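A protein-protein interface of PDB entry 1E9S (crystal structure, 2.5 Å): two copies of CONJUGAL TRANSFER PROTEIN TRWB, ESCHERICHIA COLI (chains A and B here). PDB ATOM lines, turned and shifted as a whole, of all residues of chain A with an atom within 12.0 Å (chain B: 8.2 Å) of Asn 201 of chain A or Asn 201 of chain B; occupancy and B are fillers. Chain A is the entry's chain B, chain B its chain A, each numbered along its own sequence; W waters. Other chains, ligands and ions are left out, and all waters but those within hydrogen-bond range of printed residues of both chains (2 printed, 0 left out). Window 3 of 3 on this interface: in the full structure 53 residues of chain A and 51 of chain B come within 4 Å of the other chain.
Of the 22 printed residues of chain A, 6 touch a printed residue of chain B. Along chain A the printed residues that touch a printed residue of chain B span positions 198 to 203. Of the 14 printed residues of chain B, 4 touch a printed residue of chain A. Among the printed residues, 7 pairs touch across the chains.
Among the printed residues, pairs that only touch across the chains: Ala 198 of chain A with Phe 181 of chain B (3.9 Å), Gly 199 of chain A with Phe 181 of chain B (3.3 Å), Asn 201 of chain A with Asn 201 of chain B (3.7 Å), Glu 202 of chain A with Lys 205 of chain B (3.8 Å), Glu 202 of chain A with Thr 208 of chain B (3.6 Å) and Ala 203 of chain A with Thr 208 of chain B (3.7 Å).
Asn 201 of chain A touches just one residue of chain B: Asn 201. Of the printed residues of chain A, Asn 201 of chain B touches Asn 201 (3.7 Å). Ser 200 of chain A touches just one residue of chain B: Thr 208. No residue of chain A comes within 4 Å of Ser 200 of chain B. No residue of chain A comes within 4 Å of Glu 202 of chain B. No residue of chain A comes within 4 Å of Ser 204 of chain B. Of the printed residues of chain A, Lys 205 of chain B touches Glu 202. Printed residues of chain B within 4 Å of Ala 203 of chain A: Thr 208 (3.7 Å). Printed residues of chain A within 4 Å of Phe 181 of chain B: Ala 198 (3.9 Å) and Gly 199 (3.3 Å). Printed residues of chain A within 4 Å of Thr 208 of chain B: Ser 200 (2.5 Å), Glu 202 (3.6 Å) and Ala 203 (3.7 Å). Of the printed residues of chain B, Ala 198 of chain A touches Phe 181. Printed residues of chain B within 4 Å of Glu 202 of chain A: Lys 205 (3.8 Å) and Thr 208 (3.6 Å). The nearest residue of chain B that does not touch Asn 201 of chain A is Ser 204 of chain B (5.8 Å). The nearest printed residue of chain B that does not touch Gly 199 of chain A is Arg 185 of chain B (4.6 Å).
O of Ser 200 of chain A is in hydrogen-bond range of OG of Ser 204 of chain A (3.3 Å). The side-chain hydroxyl of Ser 200 of chain A sits at hydrogen-bond distance from the backbone NH of Ala 203 of chain A (3.1 Å). OG of Ser 200 of chain A sits close to N of Glu 202 of chain A, 3.3 Å away. The side-chain hydroxyl of Thr 208 of chain B is in hydrogen-bond range of the backbone carbonyl oxygen of Ser 204 of chain B, 3.1 Å away.
OG1 of Thr 208 of chain B lies within hydrogen-bond range of OG of Ser 200 of chain A (2.5 Å).
Ala 198 of chain A touches Phe 181 of chain B, but with the chains exchanged Phe 181 of chain A does not touch Ala 198 of chain B (20.6 Å). Gly 199 of chain A touches Phe 181 of chain B, but with the chains exchanged Phe 181 of chain A does not touch Gly 199 of chain B (20.8 Å). Glu 202 of chain A touches Lys 205 of chain B, but with the chains exchanged Lys 205 of chain A does not touch Glu 202 of chain B (10.3 Å). Ala 203 of chain A touches Thr 208 of chain B, but with the chains exchanged Thr 208 of chain A does not touch Ala 203 of chain B (18.0 Å). Of the 7 pairs that touch across the chains among the printed residues, 1 has its exchanged pair printed and touching as well.
Water W2 bridges O of Leu 196 of chain A (2.9 Å) and O of Thr 208 of chain B (3.2 Å). Water W1 bridges the side-chain amide oxygen (OD1) of Asn 201 of chain B (3.1 Å) and the backbone NH (N) of Asn 201 of chain A (3.4 Å).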
ATOM      1  N   GLU A 145       6.389  -9.852  -9.231  1.00  0.00           N
ATOM      2  CA  GLU A 145       6.338  -8.883 -10.322  1.00  0.00           C
ATOM      3  C   GLU A 145       5.146  -7.976 -10.016  1.00  0.00           C
ATOM      4  O   GLU A 145       5.280  -6.744  -9.996  1.00  0.00           O
ATOM      5  CB  GLU A 145       6.135  -9.580 -11.675  1.00  0.00           C
ATOM      6  CG  GLU A 145       6.055  -8.632 -12.884  1.00  0.00           C
ATOM      7  CD  GLU A 145       5.564  -9.318 -14.167  1.00  0.00           C
ATOM      8  OE1 GLU A 145       5.214 -10.522 -14.121  1.00  0.00           O
ATOM      9  OE2 GLU A 145       5.523  -8.647 -15.227  1.00  0.00           O
ATOM     10  N   TRP A 146       3.989  -8.590  -9.757  1.00  0.00           N
ATOM     11  CA  TRP A 146       2.774  -7.835  -9.430  1.00  0.00           C
ATOM     12  C   TRP A 146       2.980  -6.989  -8.176  1.00  0.00           C
ATOM     13  O   TRP A 146       2.521  -5.846  -8.116  1.00  0.00           O
ATOM     14  CB  TRP A 146       1.557  -8.748  -9.179  1.00  0.00           C
ATOM     15  CG  TRP A 146       1.248  -9.726 -10.260  1.00  0.00           C
ATOM     16  CD1 TRP A 146       1.531  -9.605 -11.594  1.00  0.00           C
ATOM     17  CD2 TRP A 146       0.642 -11.019 -10.094  1.00  0.00           C
ATOM     18  NE1 TRP A 146       1.153 -10.747 -12.269  1.00  0.00           N
ATOM     19  CE2 TRP A 146       0.606 -11.631 -11.373  1.00  0.00           C
ATOM     20  CE3 TRP A 146       0.130 -11.722  -8.991  1.00  0.00           C
ATOM     21  CZ2 TRP A 146       0.077 -12.924 -11.573  1.00  0.00           C
ATOM     22  CZ3 TRP A 146      -0.396 -13.002  -9.195  1.00  0.00           C
ATOM     23  CH2 TRP A 146      -0.416 -13.586 -10.478  1.00  0.00           C
ATOM     24  N   TYR A 149       4.749  -3.806  -8.941  1.00  0.00           N
ATOM     25  CA  TYR A 149       3.849  -2.836  -9.552  1.00  0.00           C
ATOM     26  C   TYR A 149       3.017  -2.224  -8.436  1.00  0.00           C
ATOM     27  O   TYR A 149       2.752  -1.024  -8.429  1.00  0.00           O
ATOM     28  CB  TYR A 149       2.919  -3.527 -10.552  1.00  0.00           C
ATOM     29  CG  TYR A 149       3.627  -4.135 -11.731  1.00  0.00           C
ATOM     30  CD1 TYR A 149       4.717  -3.497 -12.309  1.00  0.00           C
ATOM     31  CD2 TYR A 149       3.231  -5.367 -12.246  1.00  0.00           C
ATOM     32  CE1 TYR A 149       5.405  -4.070 -13.367  1.00  0.00           C
ATOM     33  CE2 TYR A 149       3.917  -5.951 -13.305  1.00  0.00           C
ATOM     34  CZ  TYR A 149       5.004  -5.293 -13.858  1.00  0.00           C
ATOM     35  OH  TYR A 149       5.702  -5.852 -14.901  1.00  0.00           O
ATOM     36  N   PHE A 181     -10.015   3.613 -13.614  1.00  0.00           N
ATOM     37  CA  PHE A 181      -8.735   3.515 -14.277  1.00  0.00           C
ATOM     38  C   PHE A 181      -8.266   4.877 -14.763  1.00  0.00           C
ATOM     39  O   PHE A 181      -7.142   5.290 -14.476  1.00  0.00           O
ATOM     40  CB  PHE A 181      -8.866   2.574 -15.461  1.00  0.00           C
ATOM     41  CG  PHE A 181      -7.764   1.579 -15.565  1.00  0.00           C
ATOM     42  CD1 PHE A 181      -7.550   0.654 -14.547  1.00  0.00           C
ATOM     43  CD2 PHE A 181      -6.964   1.533 -16.700  1.00  0.00           C
ATOM     44  CE1 PHE A 181      -6.556  -0.309 -14.655  1.00  0.00           C
ATOM     45  CE2 PHE A 181      -5.963   0.573 -16.822  1.00  0.00           C
ATOM     46  CZ  PHE A 181      -5.758  -0.352 -15.795  1.00  0.00           C
ATOM     47  N   ARG A 185      -5.234   7.133 -13.410  1.00  0.00           N
ATOM     48  CA  ARG A 185      -4.201   7.515 -14.362  1.00  0.00           C
ATOM     49  C   ARG A 185      -4.022   9.019 -14.332  1.00  0.00           C
ATOM     50  O   ARG A 185      -2.897   9.519 -14.425  1.00  0.00           O
ATOM     51  CB  ARG A 185      -4.582   7.079 -15.770  1.00  0.00           C
ATOM     52  CG  ARG A 185      -4.205   5.647 -16.129  1.00  0.00           C
ATOM     53  CD  ARG A 185      -3.480   5.667 -17.460  1.00  0.00           C
ATOM     54  NE  ARG A 185      -3.105   4.351 -17.966  1.00  0.00           N
ATOM     55  CZ  ARG A 185      -3.964   3.412 -18.346  1.00  0.00           C
ATOM     56  NH1 ARG A 185      -5.274   3.628 -18.266  1.00  0.00           N
ATOM     57  NH2 ARG A 185      -3.508   2.250 -18.800  1.00  0.00           N
ATOM     58  N   SER A 195       3.929   7.864 -16.606  1.00  0.00           N
ATOM     59  CA  SER A 195       4.109   7.167 -17.876  1.00  0.00           C
ATOM     60  C   SER A 195       4.369   5.669 -17.752  1.00  0.00           C
ATOM     61  O   SER A 195       4.204   4.927 -18.718  1.00  0.00           O
ATOM     62  CB  SER A 195       5.243   7.810 -18.676  1.00  0.00           C
ATOM     63  OG  SER A 195       4.879   9.100 -19.121  1.00  0.00           O
ATOM     64  N   LEU A 196       4.776   5.221 -16.572  1.00  0.00           N
ATOM     65  CA  LEU A 196       5.045   3.812 -16.378  1.00  0.00           C
ATOM     66  C   LEU A 196       3.790   2.959 -16.522  1.00  0.00           C
ATOM     67  O   LEU A 196       3.844   1.862 -17.071  1.00  0.00           O
ATOM     68  CB  LEU A 196       5.690   3.582 -15.014  1.00  0.00           C
ATOM     69  CG  LEU A 196       7.079   4.189 -14.807  1.00  0.00           C
ATOM     70  CD1 LEU A 196       7.633   3.645 -13.534  1.00  0.00           C
ATOM     71  CD2 LEU A 196       8.010   3.842 -15.939  1.00  0.00           C
ATOM     72  N   PHE A 197       2.659   3.470 -16.046  1.00  0.00           N
ATOM     73  CA  PHE A 197       1.394   2.742 -16.128  1.00  0.00           C
ATOM     74  C   PHE A 197       0.509   3.143 -17.306  1.00  0.00           C
ATOM     75  O   PHE A 197      -0.701   2.939 -17.270  1.00  0.00           O
ATOM     76  CB  PHE A 197       0.607   2.922 -14.826  1.00  0.00           C
ATOM     77  CG  PHE A 197       1.171   2.157 -13.669  1.00  0.00           C
ATOM     78  CD1 PHE A 197       1.345   0.780 -13.748  1.00  0.00           C
ATOM     79  CD2 PHE A 197       1.504   2.801 -12.490  1.00  0.00           C
ATOM     80  CE1 PHE A 197       1.843   0.054 -12.663  1.00  0.00           C
ATOM     81  CE2 PHE A 197       2.002   2.084 -11.401  1.00  0.00           C
ATOM     82  CZ  PHE A 197       2.171   0.705 -11.490  1.00  0.00           C
ATOM     83  N   ALA A 198       1.101   3.708 -18.352  1.00  0.00           N
ATOM     84  CA  ALA A 198       0.325   4.120 -19.515  1.00  0.00           C
ATOM     85  C   ALA A 198       1.086   3.910 -20.826  1.00  0.00           C
ATOM     86  O   ALA A 198       2.297   3.690 -20.819  1.00  0.00           O
ATOM     87  CB  ALA A 198      -0.073   5.578 -19.376  1.00  0.00           C
ATOM     88  N   GLY A 199       0.366   3.953 -21.945  1.00  0.00           N
ATOM     89  CA  GLY A 199       1.006   3.802 -23.240  1.00  0.00           C
ATOM     90  C   GLY A 199       0.953   2.451 -23.934  1.00  0.00           C
ATOM     91  O   GLY A 199       1.351   2.348 -25.104  1.00  0.00           O
ATOM     92  N   SER A 200       0.489   1.410 -23.246  1.00  0.00           N
ATOM     93  CA  SER A 200       0.403   0.091 -23.877  1.00  0.00           C
ATOM     94  C   SER A 200      -0.511  -0.852 -23.112  1.00  0.00           C
ATOM     95  O   SER A 200      -0.981  -0.524 -22.020  1.00  0.00           O
ATOM     96  CB  SER A 200       1.797  -0.540 -24.010  1.00  0.00           C
ATOM     97  OG  SER A 200       2.260  -1.067 -22.778  1.00  0.00           O
ATOM     98  N   ASN A 201      -0.780  -2.017 -23.695  1.00  0.00           N
ATOM     99  CA  ASN A 201      -1.623  -2.997 -23.028  1.00  0.00           C
ATOM    100  C   ASN A 201      -0.873  -3.506 -21.813  1.00  0.00           C
ATOM    101  O   ASN A 201      -1.458  -3.709 -20.753  1.00  0.00           O
ATOM    102  CB  ASN A 201      -1.941  -4.183 -23.940  1.00  0.00           C
ATOM    103  CG  ASN A 201      -2.995  -3.861 -24.978  1.00  0.00           C
ATOM    104  OD1 ASN A 201      -3.815  -2.960 -24.795  1.00  0.00           O
ATOM    105  ND2 ASN A 201      -2.998  -4.621 -26.065  1.00  0.00           N
ATOM    106  N   GLU A 202       0.430  -3.713 -21.981  1.00  0.00           N
ATOM    107  CA  GLU A 202       1.279  -4.203 -20.909  1.00  0.00           C
ATOM    108  C   GLU A 202       1.277  -3.237 -19.719  1.00  0.00           C
ATOM    109  O   GLU A 202       1.153  -3.673 -18.577  1.00  0.00           O
ATOM    110  CB  GLU A 202       2.702  -4.429 -21.434  1.00  0.00           C
ATOM    111  CG  GLU A 202       3.707  -4.921 -20.392  1.00  0.00           C
ATOM    112  CD  GLU A 202       3.379  -6.300 -19.833  1.00  0.00           C
ATOM    113  OE1 GLU A 202       2.383  -6.918 -20.264  1.00  0.00           O
ATOM    114  OE2 GLU A 202       4.133  -6.769 -18.953  1.00  0.00           O
ATOM    115  N   ALA A 203       1.405  -1.937 -19.975  1.00  0.00           N
ATOM    116  CA  ALA A 203       1.384  -0.951 -18.893  1.00  0.00           C
ATOM    117  C   ALA A 203       0.046  -1.032 -18.142  1.00  0.00           C
ATOM    118  O   ALA A 203       0.004  -0.880 -16.919  1.00  0.00           O
ATOM    119  CB  ALA A 203       1.591   0.455 -19.456  1.00  0.00           C
ATOM    120  N   SER A 204      -1.039  -1.266 -18.887  1.00  0.00           N
ATOM    121  CA  SER A 204      -2.389  -1.397 -18.322  1.00  0.00           C
ATOM    122  C   SER A 204      -2.524  -2.660 -17.475  1.00  0.00           C
ATOM    123  O   SER A 204      -3.171  -2.646 -16.429  1.00  0.00           O
ATOM    124  CB  SER A 204      -3.428  -1.451 -19.432  1.00  0.00           C
ATOM    125  OG  SER A 204      -3.577  -0.183 -20.032  1.00  0.00           O
ATOM    126  N   LYS A 205      -1.934  -3.753 -17.960  1.00  0.00           N
ATOM    127  CA  LYS A 205      -1.945  -5.043 -17.271  1.00  0.00           C
ATOM    128  C   LYS A 205      -1.214  -4.894 -15.946  1.00  0.00           C
ATOM    129  O   LYS A 205      -1.659  -5.397 -14.919  1.00  0.00           O
ATOM    130  CB  LYS A 205      -1.249  -6.096 -18.132  1.00  0.00           C
ATOM    131  CG  LYS A 205      -1.063  -7.448 -17.464  1.00  0.00           C
ATOM    132  CD  LYS A 205      -0.564  -8.485 -18.475  1.00  0.00           C
ATOM    133  CE  LYS A 205      -0.353  -9.871 -17.847  1.00  0.00           C
ATOM    134  NZ  LYS A 205       0.755  -9.926 -16.835  1.00  0.00           N
ATOM    135  N   ALA A 206      -0.087  -4.189 -15.990  1.00  0.00           N
ATOM    136  CA  ALA A 206       0.737  -3.927 -14.822  1.00  0.00           C
ATOM    137  C   ALA A 206      -0.034  -3.093 -13.800  1.00  0.00           C
ATOM    138  O   ALA A 206      -0.029  -3.390 -12.609  1.00  0.00           O
ATOM    139  CB  ALA A 206       1.994  -3.204 -15.252  1.00  0.00           C
ATOM    140  N   LEU A 207      -0.699  -2.042 -14.264  1.00  0.00           N
ATOM    141  CA  LEU A 207      -1.483  -1.186 -13.375  1.00  0.00           C
ATOM    142  C   LEU A 207      -2.598  -2.023 -12.728  1.00  0.00           C
ATOM    143  O   LEU A 207      -2.818  -1.913 -11.520  1.00  0.00           O
ATOM    144  CB  LEU A 207      -2.071  -0.004 -14.168  1.00  0.00           C
ATOM    145  CG  LEU A 207      -2.594   1.288 -13.517  1.00  0.00           C
ATOM    146  CD1 LEU A 207      -4.084   1.281 -13.465  1.00  0.00           C
ATOM    147  CD2 LEU A 207      -1.994   1.458 -12.138  1.00  0.00           C
ATOM    148  N   THR A 208      -3.283  -2.857 -13.524  1.00  0.00           N
ATOM    149  CA  THR A 208      -4.362  -3.726 -13.030  1.00  0.00           C
ATOM    150  C   THR A 208      -3.828  -4.632 -11.932  1.00  0.00           C
ATOM    151  O   THR A 208      -4.504  -4.855 -10.930  1.00  0.00           O
ATOM    152  CB  THR A 208      -4.947  -4.647 -14.132  1.00  0.00           C
ATOM    153  OG1 THR A 208      -5.528  -3.860 -15.177  1.00  0.00           O
ATOM    154  CG2 THR A 208      -6.019  -5.555 -13.547  1.00  0.00           C
ATOM    155  N   SER A 209      -2.622  -5.159 -12.131  1.00  0.00           N
ATOM    156  CA  SER A 209      -1.985  -6.020 -11.141  1.00  0.00           C
ATOM    157  C   SER A 209      -1.711  -5.272  -9.851  1.00  0.00           C
ATOM    158  O   SER A 209      -1.931  -5.806  -8.764  1.00  0.00           O
ATOM    159  CB  SER A 209      -0.676  -6.568 -11.681  1.00  0.00           C
ATOM    160  OG  SER A 209      -0.946  -7.486 -12.710  1.00  0.00           O
ATOM    161  N   ALA A 210      -1.223  -4.041  -9.966  1.00  0.00           N
ATOM    162  CA  ALA A 210      -0.921  -3.227  -8.794  1.00  0.00           C
ATOM    163  C   ALA A 210      -2.174  -2.998  -7.957  1.00  0.00           C
ATOM    164  O   ALA A 210      -2.136  -3.057  -6.737  1.00  0.00           O
ATOM    165  CB  ALA A 210      -0.338  -1.898  -9.228  1.00  0.00           C
ATOM    166  N   ARG A 211      -3.290  -2.746  -8.626  1.00  0.00           N
ATOM    167  CA  ARG A 211      -4.564  -2.496  -7.963  1.00  0.00           C
ATOM    168  C   ARG A 211      -5.004  -3.710  -7.171  1.00  0.00           C
ATOM    169  O   ARG A 211      -5.456  -3.585  -6.032  1.00  0.00           O
ATOM    170  CB  ARG A 211      -5.629  -2.145  -9.005  1.00  0.00           C
ATOM    171  CG  ARG A 211      -5.227  -0.981  -9.888  1.00  0.00           C
ATOM    172  CD  ARG A 211      -5.936   0.280  -9.504  1.00  0.00           C
ATOM    173  NE  ARG A 211      -7.211   0.386 -10.194  1.00  0.00           N
ATOM    174  CZ  ARG A 211      -8.100   1.345  -9.971  1.00  0.00           C
ATOM    175  NH1 ARG A 211      -7.859   2.291  -9.072  1.00  0.00           N
ATOM    176  NH2 ARG A 211      -9.236   1.351 -10.651  1.00  0.00           N
ATOM    177  N   PHE B 181       4.827   7.648 -24.045  1.00  0.00           N
ATOM    178  CA  PHE B 181       5.207   6.596 -24.967  1.00  0.00           C
ATOM    179  C   PHE B 181       5.507   7.144 -26.350  1.00  0.00           C
ATOM    180  O   PHE B 181       6.540   6.835 -26.931  1.00  0.00           O
ATOM    181  CB  PHE B 181       4.090   5.567 -25.055  1.00  0.00           C
ATOM    182  CG  PHE B 181       4.538   4.180 -24.770  1.00  0.00           C
ATOM    183  CD1 PHE B 181       5.082   3.848 -23.518  1.00  0.00           C
ATOM    184  CD2 PHE B 181       4.427   3.197 -25.749  1.00  0.00           C
ATOM    185  CE1 PHE B 181       5.512   2.555 -23.245  1.00  0.00           C
ATOM    186  CE2 PHE B 181       4.851   1.895 -25.496  1.00  0.00           C
ATOM    187  CZ  PHE B 181       5.397   1.570 -24.239  1.00  0.00           C
ATOM    188  N   ARG B 185       9.082   7.247 -28.352  1.00  0.00           N
ATOM    189  CA  ARG B 185       9.170   6.637 -29.669  1.00  0.00           C
ATOM    190  C   ARG B 185       9.715   7.657 -30.660  1.00  0.00           C
ATOM    191  O   ARG B 185      10.540   7.345 -31.513  1.00  0.00           O
ATOM    192  CB  ARG B 185       7.793   6.180 -30.126  1.00  0.00           C
ATOM    193  CG  ARG B 185       7.169   5.116 -29.271  1.00  0.00           C
ATOM    194  CD  ARG B 185       7.214   3.778 -29.972  1.00  0.00           C
ATOM    195  NE  ARG B 185       6.274   2.825 -29.383  1.00  0.00           N
ATOM    196  CZ  ARG B 185       4.972   3.052 -29.239  1.00  0.00           C
ATOM    197  NH1 ARG B 185       4.440   4.207 -29.638  1.00  0.00           N
ATOM    198  NH2 ARG B 185       4.200   2.125 -28.693  1.00  0.00           N
ATOM    199  N   PHE B 197      11.143  -1.081 -31.145  1.00  0.00           N
ATOM    200  CA  PHE B 197      10.120  -0.823 -30.138  1.00  0.00           C
ATOM    201  C   PHE B 197       8.805  -0.301 -30.712  1.00  0.00           C
ATOM    202  O   PHE B 197       8.015   0.319 -30.000  1.00  0.00           O
ATOM    203  CB  PHE B 197      10.643   0.176 -29.098  1.00  0.00           C
ATOM    204  CG  PHE B 197      11.597  -0.417 -28.104  1.00  0.00           C
ATOM    205  CD1 PHE B 197      11.282  -1.593 -27.428  1.00  0.00           C
ATOM    206  CD2 PHE B 197      12.816   0.194 -27.851  1.00  0.00           C
ATOM    207  CE1 PHE B 197      12.180  -2.155 -26.517  1.00  0.00           C
ATOM    208  CE2 PHE B 197      13.715  -0.357 -26.945  1.00  0.00           C
ATOM    209  CZ  PHE B 197      13.399  -1.535 -26.277  1.00  0.00           C
ATOM    210  N   ALA B 198       8.560  -0.548 -31.991  1.00  0.00           N
ATOM    211  CA  ALA B 198       7.318  -0.095 -32.612  1.00  0.00           C
ATOM    212  C   ALA B 198       6.818  -1.068 -33.687  1.00  0.00           C
ATOM    213  O   ALA B 198       7.574  -1.921 -34.181  1.00  0.00           O
ATOM    214  CB  ALA B 198       7.523   1.280 -33.212  1.00  0.00           C
ATOM    215  N   GLY B 199       5.537  -0.961 -34.028  1.00  0.00           N
ATOM    216  CA  GLY B 199       4.997  -1.808 -35.074  1.00  0.00           C
ATOM    217  C   GLY B 199       4.120  -2.974 -34.680  1.00  0.00           C
ATOM    218  O   GLY B 199       3.534  -3.627 -35.548  1.00  0.00           O
ATOM    219  N   SER B 200       4.015  -3.254 -33.389  1.00  0.00           N
ATOM    220  CA  SER B 200       3.182  -4.366 -32.948  1.00  0.00           C
ATOM    221  C   SER B 200       2.954  -4.266 -31.462  1.00  0.00           C
ATOM    222  O   SER B 200       3.615  -3.486 -30.790  1.00  0.00           O
ATOM    223  CB  SER B 200       3.867  -5.699 -33.247  1.00  0.00           C
ATOM    224  OG  SER B 200       5.002  -5.866 -32.407  1.00  0.00           O
ATOM    225  N   ASN B 201       2.023  -5.060 -30.946  1.00  0.00           N
ATOM    226  CA  ASN B 201       1.747  -5.055 -29.516  1.00  0.00           C
ATOM    227  C   ASN B 201       2.948  -5.602 -28.757  1.00  0.00           C
ATOM    228  O   ASN B 201       3.252  -5.150 -27.657  1.00  0.00           O
ATOM    229  CB  ASN B 201       0.530  -5.917 -29.185  1.00  0.00           C
ATOM    230  CG  ASN B 201      -0.767  -5.294 -29.632  1.00  0.00           C
ATOM    231  OD1 ASN B 201      -1.120  -4.192 -29.206  1.00  0.00           O
ATOM    232  ND2 ASN B 201      -1.495  -6.001 -30.492  1.00  0.00           N
ATOM    233  N   GLU B 202       3.627  -6.581 -29.348  1.00  0.00           N
ATOM    234  CA  GLU B 202       4.783  -7.176 -28.710  1.00  0.00           C
ATOM    235  C   GLU B 202       5.892  -6.135 -28.567  1.00  0.00           C
ATOM    236  O   GLU B 202       6.547  -6.074 -27.538  1.00  0.00           O
ATOM    237  CB  GLU B 202       5.266  -8.382 -29.519  1.00  0.00           C
ATOM    238  CG  GLU B 202       6.367  -9.172 -28.838  1.00  0.00           C
ATOM    239  CD  GLU B 202       5.936  -9.755 -27.498  1.00  0.00           C
ATOM    240  OE1 GLU B 202       4.717  -9.763 -27.210  1.00  0.00           O
ATOM    241  OE2 GLU B 202       6.819 -10.206 -26.736  1.00  0.00           O
ATOM    242  N   ALA B 203       6.095  -5.316 -29.597  1.00  0.00           N
ATOM    243  CA  ALA B 203       7.120  -4.271 -29.568  1.00  0.00           C
ATOM    244  C   ALA B 203       6.801  -3.257 -28.468  1.00  0.00           C
ATOM    245  O   ALA B 203       7.689  -2.738 -27.801  1.00  0.00           O
ATOM    246  CB  ALA B 203       7.187  -3.563 -30.926  1.00  0.00           C
ATOM    247  N   SER B 204       5.517  -2.976 -28.299  1.00  0.00           N
ATOM    248  CA  SER B 204       5.052  -2.044 -27.284  1.00  0.00           C
ATOM    249  C   SER B 204       5.240  -2.657 -25.906  1.00  0.00           C
ATOM    250  O   SER B 204       5.596  -1.964 -24.952  1.00  0.00           O
ATOM    251  CB  SER B 204       3.564  -1.727 -27.480  1.00  0.00           C
ATOM    252  OG  SER B 204       3.353  -0.813 -28.536  1.00  0.00           O
ATOM    253  N   LYS B 205       4.977  -3.955 -25.797  1.00  0.00           N
ATOM    254  CA  LYS B 205       5.124  -4.657 -24.532  1.00  0.00           C
ATOM    255  C   LYS B 205       6.587  -4.615 -24.145  1.00  0.00           C
ATOM    256  O   LYS B 205       6.920  -4.317 -23.002  1.00  0.00           O
ATOM    257  CB  LYS B 205       4.667  -6.106 -24.667  1.00  0.00           C
ATOM    258  CG  LYS B 205       4.861  -6.920 -23.398  1.00  0.00           C
ATOM    259  CD  LYS B 205       4.394  -8.351 -23.603  1.00  0.00           C
ATOM    260  CE  LYS B 205       4.694  -9.227 -22.398  1.00  0.00           C
ATOM    261  NZ  LYS B 205       4.223 -10.625 -22.614  1.00  0.00           N
ATOM    262  N   ALA B 206       7.450  -4.903 -25.117  1.00  0.00           N
ATOM    263  CA  ALA B 206       8.893  -4.896 -24.923  1.00  0.00           C
ATOM    264  C   ALA B 206       9.357  -3.538 -24.416  1.00  0.00           C
ATOM    265  O   ALA B 206      10.144  -3.457 -23.484  1.00  0.00           O
ATOM    266  CB  ALA B 206       9.592  -5.229 -26.226  1.00  0.00           C
ATOM    267  N   LEU B 207       8.868  -2.469 -25.039  1.00  0.00           N
ATOM    268  CA  LEU B 207       9.223  -1.111 -24.638  1.00  0.00           C
ATOM    269  C   LEU B 207       8.753  -0.846 -23.200  1.00  0.00           C
ATOM    270  O   LEU B 207       9.476  -0.252 -22.402  1.00  0.00           O
ATOM    271  CB  LEU B 207       8.581  -0.085 -25.583  1.00  0.00           C
ATOM    272  CG  LEU B 207       9.282   1.277 -25.754  1.00  0.00           C
ATOM    273  CD1 LEU B 207       8.284   2.377 -25.565  1.00  0.00           C
ATOM    274  CD2 LEU B 207      10.425   1.447 -24.778  1.00  0.00           C
ATOM    275  N   THR B 208       7.540  -1.282 -22.875  1.00  0.00           N
ATOM    276  CA  THR B 208       7.010  -1.089 -21.537  1.00  0.00           C
ATOM    277  C   THR B 208       7.901  -1.781 -20.510  1.00  0.00           C
ATOM    278  O   THR B 208       8.180  -1.232 -19.450  1.00  0.00           O
ATOM    279  CB  THR B 208       5.584  -1.632 -21.427  1.00  0.00           C
ATOM    280  OG1 THR B 208       4.722  -0.818 -22.223  1.00  0.00           O
ATOM    281  CG2 THR B 208       5.106  -1.583 -19.998  1.00  0.00           C
HETATM  282  O   HOH W   1       0.049  -2.366 -26.955  1.00  0.00           O
HETATM  283  O   HOH W   2       6.253   1.128 -18.605  1.00  0.00           O
